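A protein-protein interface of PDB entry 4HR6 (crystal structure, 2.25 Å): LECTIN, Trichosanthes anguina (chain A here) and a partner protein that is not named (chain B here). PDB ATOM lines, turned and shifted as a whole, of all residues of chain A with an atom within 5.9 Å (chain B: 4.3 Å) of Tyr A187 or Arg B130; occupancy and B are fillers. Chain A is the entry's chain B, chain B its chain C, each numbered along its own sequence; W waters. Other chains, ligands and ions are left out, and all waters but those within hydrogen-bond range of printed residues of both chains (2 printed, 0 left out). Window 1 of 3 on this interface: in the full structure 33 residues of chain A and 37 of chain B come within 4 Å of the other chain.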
ATOM      1  N   GLN A 164     -20.880  23.372   6.919  1.00  0.00           N
ATOM      2  CA  GLN A 164     -21.030  22.291   5.930  1.00  0.00           C
ATOM      3  C   GLN A 164     -19.694  21.689   5.470  1.00  0.00           C
ATOM      4  O   GLN A 164     -19.595  21.216   4.345  1.00  0.00           O
ATOM      5  CB  GLN A 164     -21.764  22.818   4.673  1.00  0.00           C
ATOM      6  CG  GLN A 164     -23.112  23.485   4.917  1.00  0.00           C
ATOM      7  CD  GLN A 164     -24.270  22.503   4.866  1.00  0.00           C
ATOM      8  OE1 GLN A 164     -24.124  21.318   5.186  1.00  0.00           O
ATOM      9  NE2 GLN A 164     -25.432  22.994   4.450  1.00  0.00           N
ATOM     10  N   GLY A 165     -18.663  21.754   6.308  1.00  0.00           N
ATOM     11  CA  GLY A 165     -17.367  21.160   5.968  1.00  0.00           C
ATOM     12  C   GLY A 165     -16.502  22.022   5.078  1.00  0.00           C
ATOM     13  O   GLY A 165     -15.455  21.582   4.611  1.00  0.00           O
ATOM     14  N   LEU A 166     -16.923  23.264   4.863  1.00  0.00           N
ATOM     15  CA  LEU A 166     -16.147  24.203   4.086  1.00  0.00           C
ATOM     16  C   LEU A 166     -15.166  24.977   4.965  1.00  0.00           C
ATOM     17  O   LEU A 166     -15.493  25.406   6.075  1.00  0.00           O
ATOM     18  CB  LEU A 166     -17.073  25.186   3.363  1.00  0.00           C
ATOM     19  CG  LEU A 166     -17.851  24.536   2.204  1.00  0.00           C
ATOM     20  CD1 LEU A 166     -19.228  25.158   2.041  1.00  0.00           C
ATOM     21  CD2 LEU A 166     -17.065  24.643   0.911  1.00  0.00           C
ATOM     22  N   SER A 185     -12.123  22.627   1.554  1.00  0.00           N
ATOM     23  CA  SER A 185     -13.152  21.890   2.285  1.00  0.00           C
ATOM     24  C   SER A 185     -12.579  20.595   2.813  1.00  0.00           C
ATOM     25  O   SER A 185     -11.489  20.200   2.439  1.00  0.00           O
ATOM     26  CB  SER A 185     -14.351  21.573   1.374  1.00  0.00           C
ATOM     27  OG  SER A 185     -14.021  20.548   0.455  1.00  0.00           O
ATOM     28  N   ILE A 186     -13.329  19.921   3.664  1.00  0.00           N
ATOM     29  CA  ILE A 186     -12.906  18.620   4.148  1.00  0.00           C
ATOM     30  C   ILE A 186     -13.112  17.465   3.157  1.00  0.00           C
ATOM     31  O   ILE A 186     -12.669  16.363   3.427  1.00  0.00           O
ATOM     32  CB  ILE A 186     -13.659  18.210   5.406  1.00  0.00           C
ATOM     33  CG1 ILE A 186     -15.165  18.295   5.158  1.00  0.00           C
ATOM     34  CG2 ILE A 186     -13.211  19.051   6.583  1.00  0.00           C
ATOM     35  CD1 ILE A 186     -15.928  17.274   5.953  1.00  0.00           C
ATOM     36  N   TYR A 187     -13.781  17.714   2.029  1.00  0.00           N
ATOM     37  CA  TYR A 187     -14.251  16.633   1.165  1.00  0.00           C
ATOM     38  C   TYR A 187     -13.150  16.211   0.216  1.00  0.00           C
ATOM     39  O   TYR A 187     -13.411  15.951  -0.951  1.00  0.00           O
ATOM     40  CB  TYR A 187     -15.525  17.066   0.407  1.00  0.00           C
ATOM     41  CG  TYR A 187     -16.601  17.476   1.368  1.00  0.00           C
ATOM     42  CD1 TYR A 187     -17.000  18.797   1.484  1.00  0.00           C
ATOM     43  CD2 TYR A 187     -17.157  16.557   2.214  1.00  0.00           C
ATOM     44  CE1 TYR A 187     -17.967  19.181   2.393  1.00  0.00           C
ATOM     45  CE2 TYR A 187     -18.115  16.928   3.135  1.00  0.00           C
ATOM     46  CZ  TYR A 187     -18.516  18.244   3.203  1.00  0.00           C
ATOM     47  OH  TYR A 187     -19.462  18.599   4.121  1.00  0.00           O
ATOM     48  N   TYR A 188     -11.916  16.178   0.720  1.00  0.00           N
ATOM     49  CA  TYR A 188     -10.762  15.709  -0.035  1.00  0.00           C
ATOM     50  C   TYR A 188     -10.055  14.627   0.781  1.00  0.00           C
ATOM     51  O   TYR A 188      -9.819  14.806   1.985  1.00  0.00           O
ATOM     52  CB  TYR A 188      -9.805  16.848  -0.331  1.00  0.00           C
ATOM     53  CG  TYR A 188     -10.365  17.872  -1.279  1.00  0.00           C
ATOM     54  CD1 TYR A 188     -11.186  18.895  -0.815  1.00  0.00           C
ATOM     55  CD2 TYR A 188     -10.072  17.830  -2.639  1.00  0.00           C
ATOM     56  CE1 TYR A 188     -11.705  19.841  -1.673  1.00  0.00           C
ATOM     57  CE2 TYR A 188     -10.599  18.765  -3.509  1.00  0.00           C
ATOM     58  CZ  TYR A 188     -11.416  19.776  -3.017  1.00  0.00           C
ATOM     59  OH  TYR A 188     -11.952  20.734  -3.853  1.00  0.00           O
ATOM     60  N   PRO A 189      -9.740  13.486   0.145  1.00  0.00           N
ATOM     61  CA  PRO A 189      -9.099  12.433   0.935  1.00  0.00           C
ATOM     62  C   PRO A 189      -7.747  12.855   1.491  1.00  0.00           C
ATOM     63  O   PRO A 189      -7.354  12.399   2.575  1.00  0.00           O
ATOM     64  CB  PRO A 189      -8.960  11.257  -0.056  1.00  0.00           C
ATOM     65  CG  PRO A 189      -9.285  11.795  -1.397  1.00  0.00           C
ATOM     66  CD  PRO A 189     -10.115  13.024  -1.204  1.00  0.00           C
ATOM     67  N   ARG B  11     -17.270  25.357  -5.783  1.00  0.00           N
ATOM     68  CA  ARG B  11     -17.944  24.549  -6.812  1.00  0.00           C
ATOM     69  C   ARG B  11     -18.466  23.249  -6.226  1.00  0.00           C
ATOM     70  O   ARG B  11     -18.061  22.820  -5.135  1.00  0.00           O
ATOM     71  CB  ARG B  11     -17.017  24.249  -7.991  1.00  0.00           C
ATOM     72  CG  ARG B  11     -16.668  25.471  -8.828  1.00  0.00           C
ATOM     73  CD  ARG B  11     -15.198  25.520  -9.198  1.00  0.00           C
ATOM     74  NE  ARG B  11     -14.958  25.243 -10.599  1.00  0.00           N
ATOM     75  CZ  ARG B  11     -13.765  25.001 -11.135  1.00  0.00           C
ATOM     76  NH1 ARG B  11     -12.670  24.979 -10.389  1.00  0.00           N
ATOM     77  NH2 ARG B  11     -13.676  24.766 -12.440  1.00  0.00           N
ATOM     78  N   ILE B  12     -19.408  22.650  -6.948  1.00  0.00           N
ATOM     79  CA  ILE B  12     -19.922  21.331  -6.616  1.00  0.00           C
ATOM     80  C   ILE B  12     -19.704  20.472  -7.850  1.00  0.00           C
ATOM     81  O   ILE B  12     -20.250  20.770  -8.916  1.00  0.00           O
ATOM     82  CB  ILE B  12     -21.413  21.367  -6.264  1.00  0.00           C
ATOM     83  CG1 ILE B  12     -21.686  22.465  -5.240  1.00  0.00           C
ATOM     84  CG2 ILE B  12     -21.875  20.015  -5.732  1.00  0.00           C
ATOM     85  CD1 ILE B  12     -23.127  22.544  -4.798  1.00  0.00           C
ATOM     86  N   SER B  13     -18.873  19.435  -7.723  1.00  0.00           N
ATOM     87  CA  SER B  13     -18.635  18.518  -8.829  1.00  0.00           C
ATOM     88  C   SER B  13     -19.096  17.119  -8.453  1.00  0.00           C
ATOM     89  O   SER B  13     -19.329  16.822  -7.274  1.00  0.00           O
ATOM     90  CB  SER B  13     -17.171  18.546  -9.265  1.00  0.00           C
ATOM     91  OG  SER B  13     -16.304  18.009  -8.288  1.00  0.00           O
ATOM     92  N   VAL B  89     -24.880  18.724   3.607  1.00  0.00           N
ATOM     93  CA  VAL B  89     -23.812  17.961   2.952  1.00  0.00           C
ATOM     94  C   VAL B  89     -23.203  16.993   3.972  1.00  0.00           C
ATOM     95  O   VAL B  89     -22.903  17.383   5.109  1.00  0.00           O
ATOM     96  CB  VAL B  89     -22.728  18.905   2.400  1.00  0.00           C
ATOM     97  CG1 VAL B  89     -21.677  18.155   1.595  1.00  0.00           C
ATOM     98  CG2 VAL B  89     -23.369  19.986   1.544  1.00  0.00           C
ATOM     99  N   SER B  90     -23.056  15.730   3.569  1.00  0.00           N
ATOM    100  CA  SER B  90     -22.492  14.666   4.425  1.00  0.00           C
ATOM    101  C   SER B  90     -21.070  14.354   3.999  1.00  0.00           C
ATOM    102  O   SER B  90     -20.689  14.572   2.839  1.00  0.00           O
ATOM    103  CB  SER B  90     -23.314  13.367   4.327  1.00  0.00           C
ATOM    104  OG  SER B  90     -23.025  12.648   3.116  1.00  0.00           O
ATOM    105  N   VAL B  91     -20.307  13.794   4.934  1.00  0.00           N
ATOM    106  CA  VAL B  91     -18.927  13.366   4.670  1.00  0.00           C
ATOM    107  C   VAL B  91     -18.833  12.392   3.498  1.00  0.00           C
ATOM    108  O   VAL B  91     -17.846  12.393   2.770  1.00  0.00           O
ATOM    109  CB  VAL B  91     -18.291  12.716   5.924  1.00  0.00           C
ATOM    110  CG1 VAL B  91     -16.915  12.148   5.605  1.00  0.00           C
ATOM    111  CG2 VAL B  91     -18.207  13.733   7.052  1.00  0.00           C
ATOM    112  N   TRP B 129     -21.240  13.600  -4.517  1.00  0.00           N
ATOM    113  CA  TRP B 129     -20.780  14.946  -4.879  1.00  0.00           C
ATOM    114  C   TRP B 129     -19.594  15.390  -4.025  1.00  0.00           C
ATOM    115  O   TRP B 129     -19.502  15.020  -2.870  1.00  0.00           O
ATOM    116  CB  TRP B 129     -21.926  15.947  -4.706  1.00  0.00           C
ATOM    117  CG  TRP B 129     -23.173  15.549  -5.397  1.00  0.00           C
ATOM    118  CD1 TRP B 129     -24.236  14.889  -4.856  1.00  0.00           C
ATOM    119  CD2 TRP B 129     -23.493  15.781  -6.762  1.00  0.00           C
ATOM    120  NE1 TRP B 129     -25.200  14.696  -5.804  1.00  0.00           N
ATOM    121  CE2 TRP B 129     -24.768  15.232  -6.988  1.00  0.00           C
ATOM    122  CE3 TRP B 129     -22.818  16.398  -7.823  1.00  0.00           C
ATOM    123  CZ2 TRP B 129     -25.391  15.280  -8.230  1.00  0.00           C
ATOM    124  CZ3 TRP B 129     -23.435  16.449  -9.065  1.00  0.00           C
ATOM    125  CH2 TRP B 129     -24.716  15.895  -9.256  1.00  0.00           C
ATOM    126  N   ARG B 130     -18.712  16.180  -4.631  1.00  0.00           N
ATOM    127  CA  ARG B 130     -17.626  16.870  -3.954  1.00  0.00           C
ATOM    128  C   ARG B 130     -17.897  18.375  -3.919  1.00  0.00           C
ATOM    129  O   ARG B 130     -17.878  19.055  -4.967  1.00  0.00           O
ATOM    130  CB  ARG B 130     -16.300  16.648  -4.676  1.00  0.00           C
ATOM    131  CG  ARG B 130     -15.122  17.313  -3.973  1.00  0.00           C
ATOM    132  CD  ARG B 130     -13.933  17.444  -4.911  1.00  0.00           C
ATOM    133  NE  ARG B 130     -13.351  16.144  -5.241  1.00  0.00           N
ATOM    134  CZ  ARG B 130     -12.417  15.949  -6.163  1.00  0.00           C
ATOM    135  NH1 ARG B 130     -11.945  16.964  -6.876  1.00  0.00           N
ATOM    136  NH2 ARG B 130     -11.966  14.715  -6.394  1.00  0.00           N
ATOM    137  N   VAL B 131     -18.117  18.886  -2.714  1.00  0.00           N
ATOM    138  CA  VAL B 131     -18.206  20.328  -2.497  1.00  0.00           C
ATOM    139  C   VAL B 131     -16.802  20.844  -2.259  1.00  0.00           C
ATOM    140  O   VAL B 131     -16.155  20.477  -1.290  1.00  0.00           O
ATOM    141  CB  VAL B 131     -19.077  20.646  -1.282  1.00  0.00           C
ATOM    142  CG1 VAL B 131     -19.115  22.146  -1.042  1.00  0.00           C
ATOM    143  CG2 VAL B 131     -20.465  20.077  -1.487  1.00  0.00           C
ATOM    144  N   GLY B 132     -16.321  21.672  -3.163  1.00  0.00           N
ATOM    145  CA  GLY B 132     -14.954  22.115  -3.117  1.00  0.00           C
ATOM    146  C   GLY B 132     -14.545  22.674  -4.450  1.00  0.00           C
ATOM    147  O   GLY B 132     -15.148  22.361  -5.480  1.00  0.00           O
ATOM    148  N   TYR B 134     -11.518  22.531  -5.992  1.00  0.00           N
ATOM    149  CA  TYR B 134     -10.656  21.703  -6.832  1.00  0.00           C
ATOM    150  C   TYR B 134     -11.504  20.553  -7.364  1.00  0.00           C
ATOM    151  O   TYR B 134     -11.896  19.673  -6.597  1.00  0.00           O
ATOM    152  CB  TYR B 134      -9.465  21.193  -6.025  1.00  0.00           C
ATOM    153  CG  TYR B 134      -8.410  20.498  -6.827  1.00  0.00           C
ATOM    154  CD1 TYR B 134      -7.407  21.217  -7.454  1.00  0.00           C
ATOM    155  CD2 TYR B 134      -8.408  19.114  -6.949  1.00  0.00           C
ATOM    156  CE1 TYR B 134      -6.427  20.575  -8.186  1.00  0.00           C
ATOM    157  CE2 TYR B 134      -7.441  18.466  -7.683  1.00  0.00           C
ATOM    158  CZ  TYR B 134      -6.458  19.194  -8.291  1.00  0.00           C
ATOM    159  OH  TYR B 134      -5.498  18.541  -9.008  1.00  0.00           O
ATOM    160  N   VAL B 135     -11.790  20.576  -8.668  1.00  0.00           N
ATOM    161  CA  VAL B 135     -12.768  19.651  -9.270  1.00  0.00           C
ATOM    162  C   VAL B 135     -12.123  18.426  -9.916  1.00  0.00           C
ATOM    163  O   VAL B 135     -12.783  17.424 -10.149  1.00  0.00           O
ATOM    164  CB  VAL B 135     -13.684  20.357 -10.310  1.00  0.00           C
ATOM    165  CG1 VAL B 135     -14.626  21.343  -9.624  1.00  0.00           C
ATOM    166  CG2 VAL B 135     -12.869  21.063 -11.386  1.00  0.00           C
ATOM    167  N   GLN B 136     -10.829  18.509 -10.201  1.00  0.00           N
ATOM    168  CA  GLN B 136     -10.136  17.426 -10.844  1.00  0.00           C
ATOM    169  C   GLN B 136     -10.111  16.146  -9.999  1.00  0.00           C
ATOM    170  O   GLN B 136     -10.285  16.176  -8.762  1.00  0.00           O
ATOM    171  CB  GLN B 136      -8.713  17.846 -11.215  1.00  0.00           C
ATOM    172  CG  GLN B 136      -8.660  18.929 -12.285  1.00  0.00           C
ATOM    173  CD  GLN B 136      -7.244  19.353 -12.623  1.00  0.00           C
ATOM    174  OE1 GLN B 136      -6.332  18.529 -12.664  1.00  0.00           O
ATOM    175  NE2 GLN B 136      -7.051  20.649 -12.871  1.00  0.00           N
ATOM    176  N   ILE B 138      -8.324  13.084  -8.105  1.00  0.00           N
ATOM    177  CA  ILE B 138      -7.089  12.949  -7.342  1.00  0.00           C
ATOM    178  C   ILE B 138      -6.386  11.669  -7.777  1.00  0.00           C
ATOM    179  O   ILE B 138      -6.905  10.574  -7.560  1.00  0.00           O
ATOM    180  CB  ILE B 138      -7.359  12.828  -5.815  1.00  0.00           C
ATOM    181  CG1 ILE B 138      -8.197  13.997  -5.288  1.00  0.00           C
ATOM    182  CG2 ILE B 138      -6.042  12.705  -5.053  1.00  0.00           C
ATOM    183  CD1 ILE B 138      -7.608  15.349  -5.581  1.00  0.00           C
ATOM    184  N   LEU B 175      -9.349   9.190  -8.391  1.00  0.00           N
ATOM    185  CA  LEU B 175     -10.489   9.347  -7.493  1.00  0.00           C
ATOM    186  C   LEU B 175     -11.375  10.508  -7.964  1.00  0.00           C
ATOM    187  O   LEU B 175     -10.952  11.664  -7.988  1.00  0.00           O
ATOM    188  CB  LEU B 175     -10.013   9.584  -6.067  1.00  0.00           C
ATOM    189  CG  LEU B 175      -9.455   8.389  -5.284  1.00  0.00           C
ATOM    190  CD1 LEU B 175      -8.407   7.604  -6.064  1.00  0.00           C
ATOM    191  CD2 LEU B 175      -8.862   8.888  -3.978  1.00  0.00           C
ATOM    192  N   TYR B 176     -12.608  10.182  -8.330  1.00  0.00           N
ATOM    193  CA  TYR B 176     -13.526  11.149  -8.934  1.00  0.00           C
ATOM    194  C   TYR B 176     -14.471  11.704  -7.885  1.00  0.00           C
ATOM    195  O   TYR B 176     -14.727  11.065  -6.857  1.00  0.00           O
ATOM    196  CB  TYR B 176     -14.330  10.495 -10.086  1.00  0.00           C
ATOM    197  CG  TYR B 176     -13.650  10.567 -11.434  1.00  0.00           C
ATOM    198  CD1 TYR B 176     -12.426   9.962 -11.641  1.00  0.00           C
ATOM    199  CD2 TYR B 176     -14.241  11.239 -12.511  1.00  0.00           C
ATOM    200  CE1 TYR B 176     -11.779  10.027 -12.862  1.00  0.00           C
ATOM    201  CE2 TYR B 176     -13.602  11.310 -13.741  1.00  0.00           C
ATOM    202  CZ  TYR B 176     -12.368  10.698 -13.907  1.00  0.00           C
ATOM    203  OH  TYR B 176     -11.710  10.752 -15.114  1.00  0.00           O
ATOM    204  N   SER B 177     -15.009  12.888  -8.182  1.00  0.00           N
ATOM    205  CA  SER B 177     -15.890  13.626  -7.277  1.00  0.00           C
ATOM    206  C   SER B 177     -17.153  12.863  -6.930  1.00  0.00           C
ATOM    207  O   SER B 177     -17.761  13.104  -5.891  1.00  0.00           O
ATOM    208  CB  SER B 177     -16.268  14.968  -7.912  1.00  0.00           C
ATOM    209  OG  SER B 177     -15.107  15.710  -8.274  1.00  0.00           O
HETATM  210  O   HOH W   1     -23.412  19.594   7.179  1.00  0.00           O
HETATM  211  O   HOH W   2     -14.085  14.357  -3.240  1.00  0.00           O
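OE1 of Gln A164 sits at hydrogen-bond distance from N of Val B89 (3.1 Å).
The backbone carbonyl oxygen of Val B131 sits at hydrogen-bond distance from the side-chain hydroxyl of Ser A185 (2.8 Å).
The backbone NH (N) of Tyr B134 sits at hydrogen-bond distance from the side-chain hydroxyl (OH) of Tyr A188 (2.8 Å).
OH of Tyr A187 sits at hydrogen-bond distance from O of Gln A164 (2.6 Å).
O of Arg B11 lies within hydrogen-bond range of N of Gly B132 (2.9 Å).
O of Ser B13 sits at hydrogen-bond distance from N of Arg B130 (2.8 Å).
The guanidinium group of Arg B130 lies close to the backbone carbonyl oxygen of Val B135, 3.4 Å away.
The guanidinium group (NH1) of Arg B130 is in hydrogen-bond range of the backbone carbonyl oxygen (O) of Gln B136, 2.6 Å away.
The backbone NH (N) of Arg B130 sits at hydrogen-bond distance from the backbone carbonyl oxygen (O) of Ser B177 (3.5 Å).
Among the printed residues, pairs that only touch across the chains: Tyr A188 with Gly B132 (3.3 Å), Tyr A187 with Val B131 (3.4 Å), Tyr A187 with Val B89 (3.4 Å), Tyr A187 with Ser B90 (3.5 Å), Tyr A187 with Arg B130 (3.7 Å), Leu A166 with Val B131 (3.8 Å), Tyr A188 with Arg B130 (3.9 Å), Pro A189 with Leu B175 (3.9 Å) and Tyr A187 with Val B91 (3.96 Å).
Printed residues of chain A within 4 Å of Arg B130: Tyr A187 and Tyr A188.
Printed residues of chain B within 4 Å of Leu A166: Val B131.
Printed residues of chain A within 4 Å of Val B89: Gln A164 and Tyr A187.
Of the printed residues of chain B, Pro A189 touches Leu B175.
Ile A186 touches none of the printed residues of chain B.
The nearest printed residue of chain B that does not touch Tyr A187 is Gly B132 (5.5 Å).
The nearest residue of chain A that does not touch Arg B130 is Ser A185 (5.6 Å).
Of the 17 printed residues of chain B, 8 touch a printed residue of chain A.
Printed residues of chain B that touch a printed residue of chain A: Val B89, Ser B90, Val B91, Arg B130, Val B131, Gly B132, Tyr B134 and Leu B175.
Hydrophobic or aromatic side chains of chain B within 4 Å of the printed part of chain A: Val B89, Val B131, Tyr B134 and Leu B175.
Of the 8 printed residues of chain A, 6 touch a printed residue of chain B.
Hydrophobic or aromatic side chains of chain A within 4 Å of the printed part of chain B: Leu A166, Tyr A187, Tyr A188 and Pro A189.
Water W1 bridges OE1 of Gln A164 and O of Val B89.
Water W2 bridges the guanidinium group of Arg B130 (2.8 Å) and the backbone carbonyl oxygen of Tyr A187 (2.9 Å).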
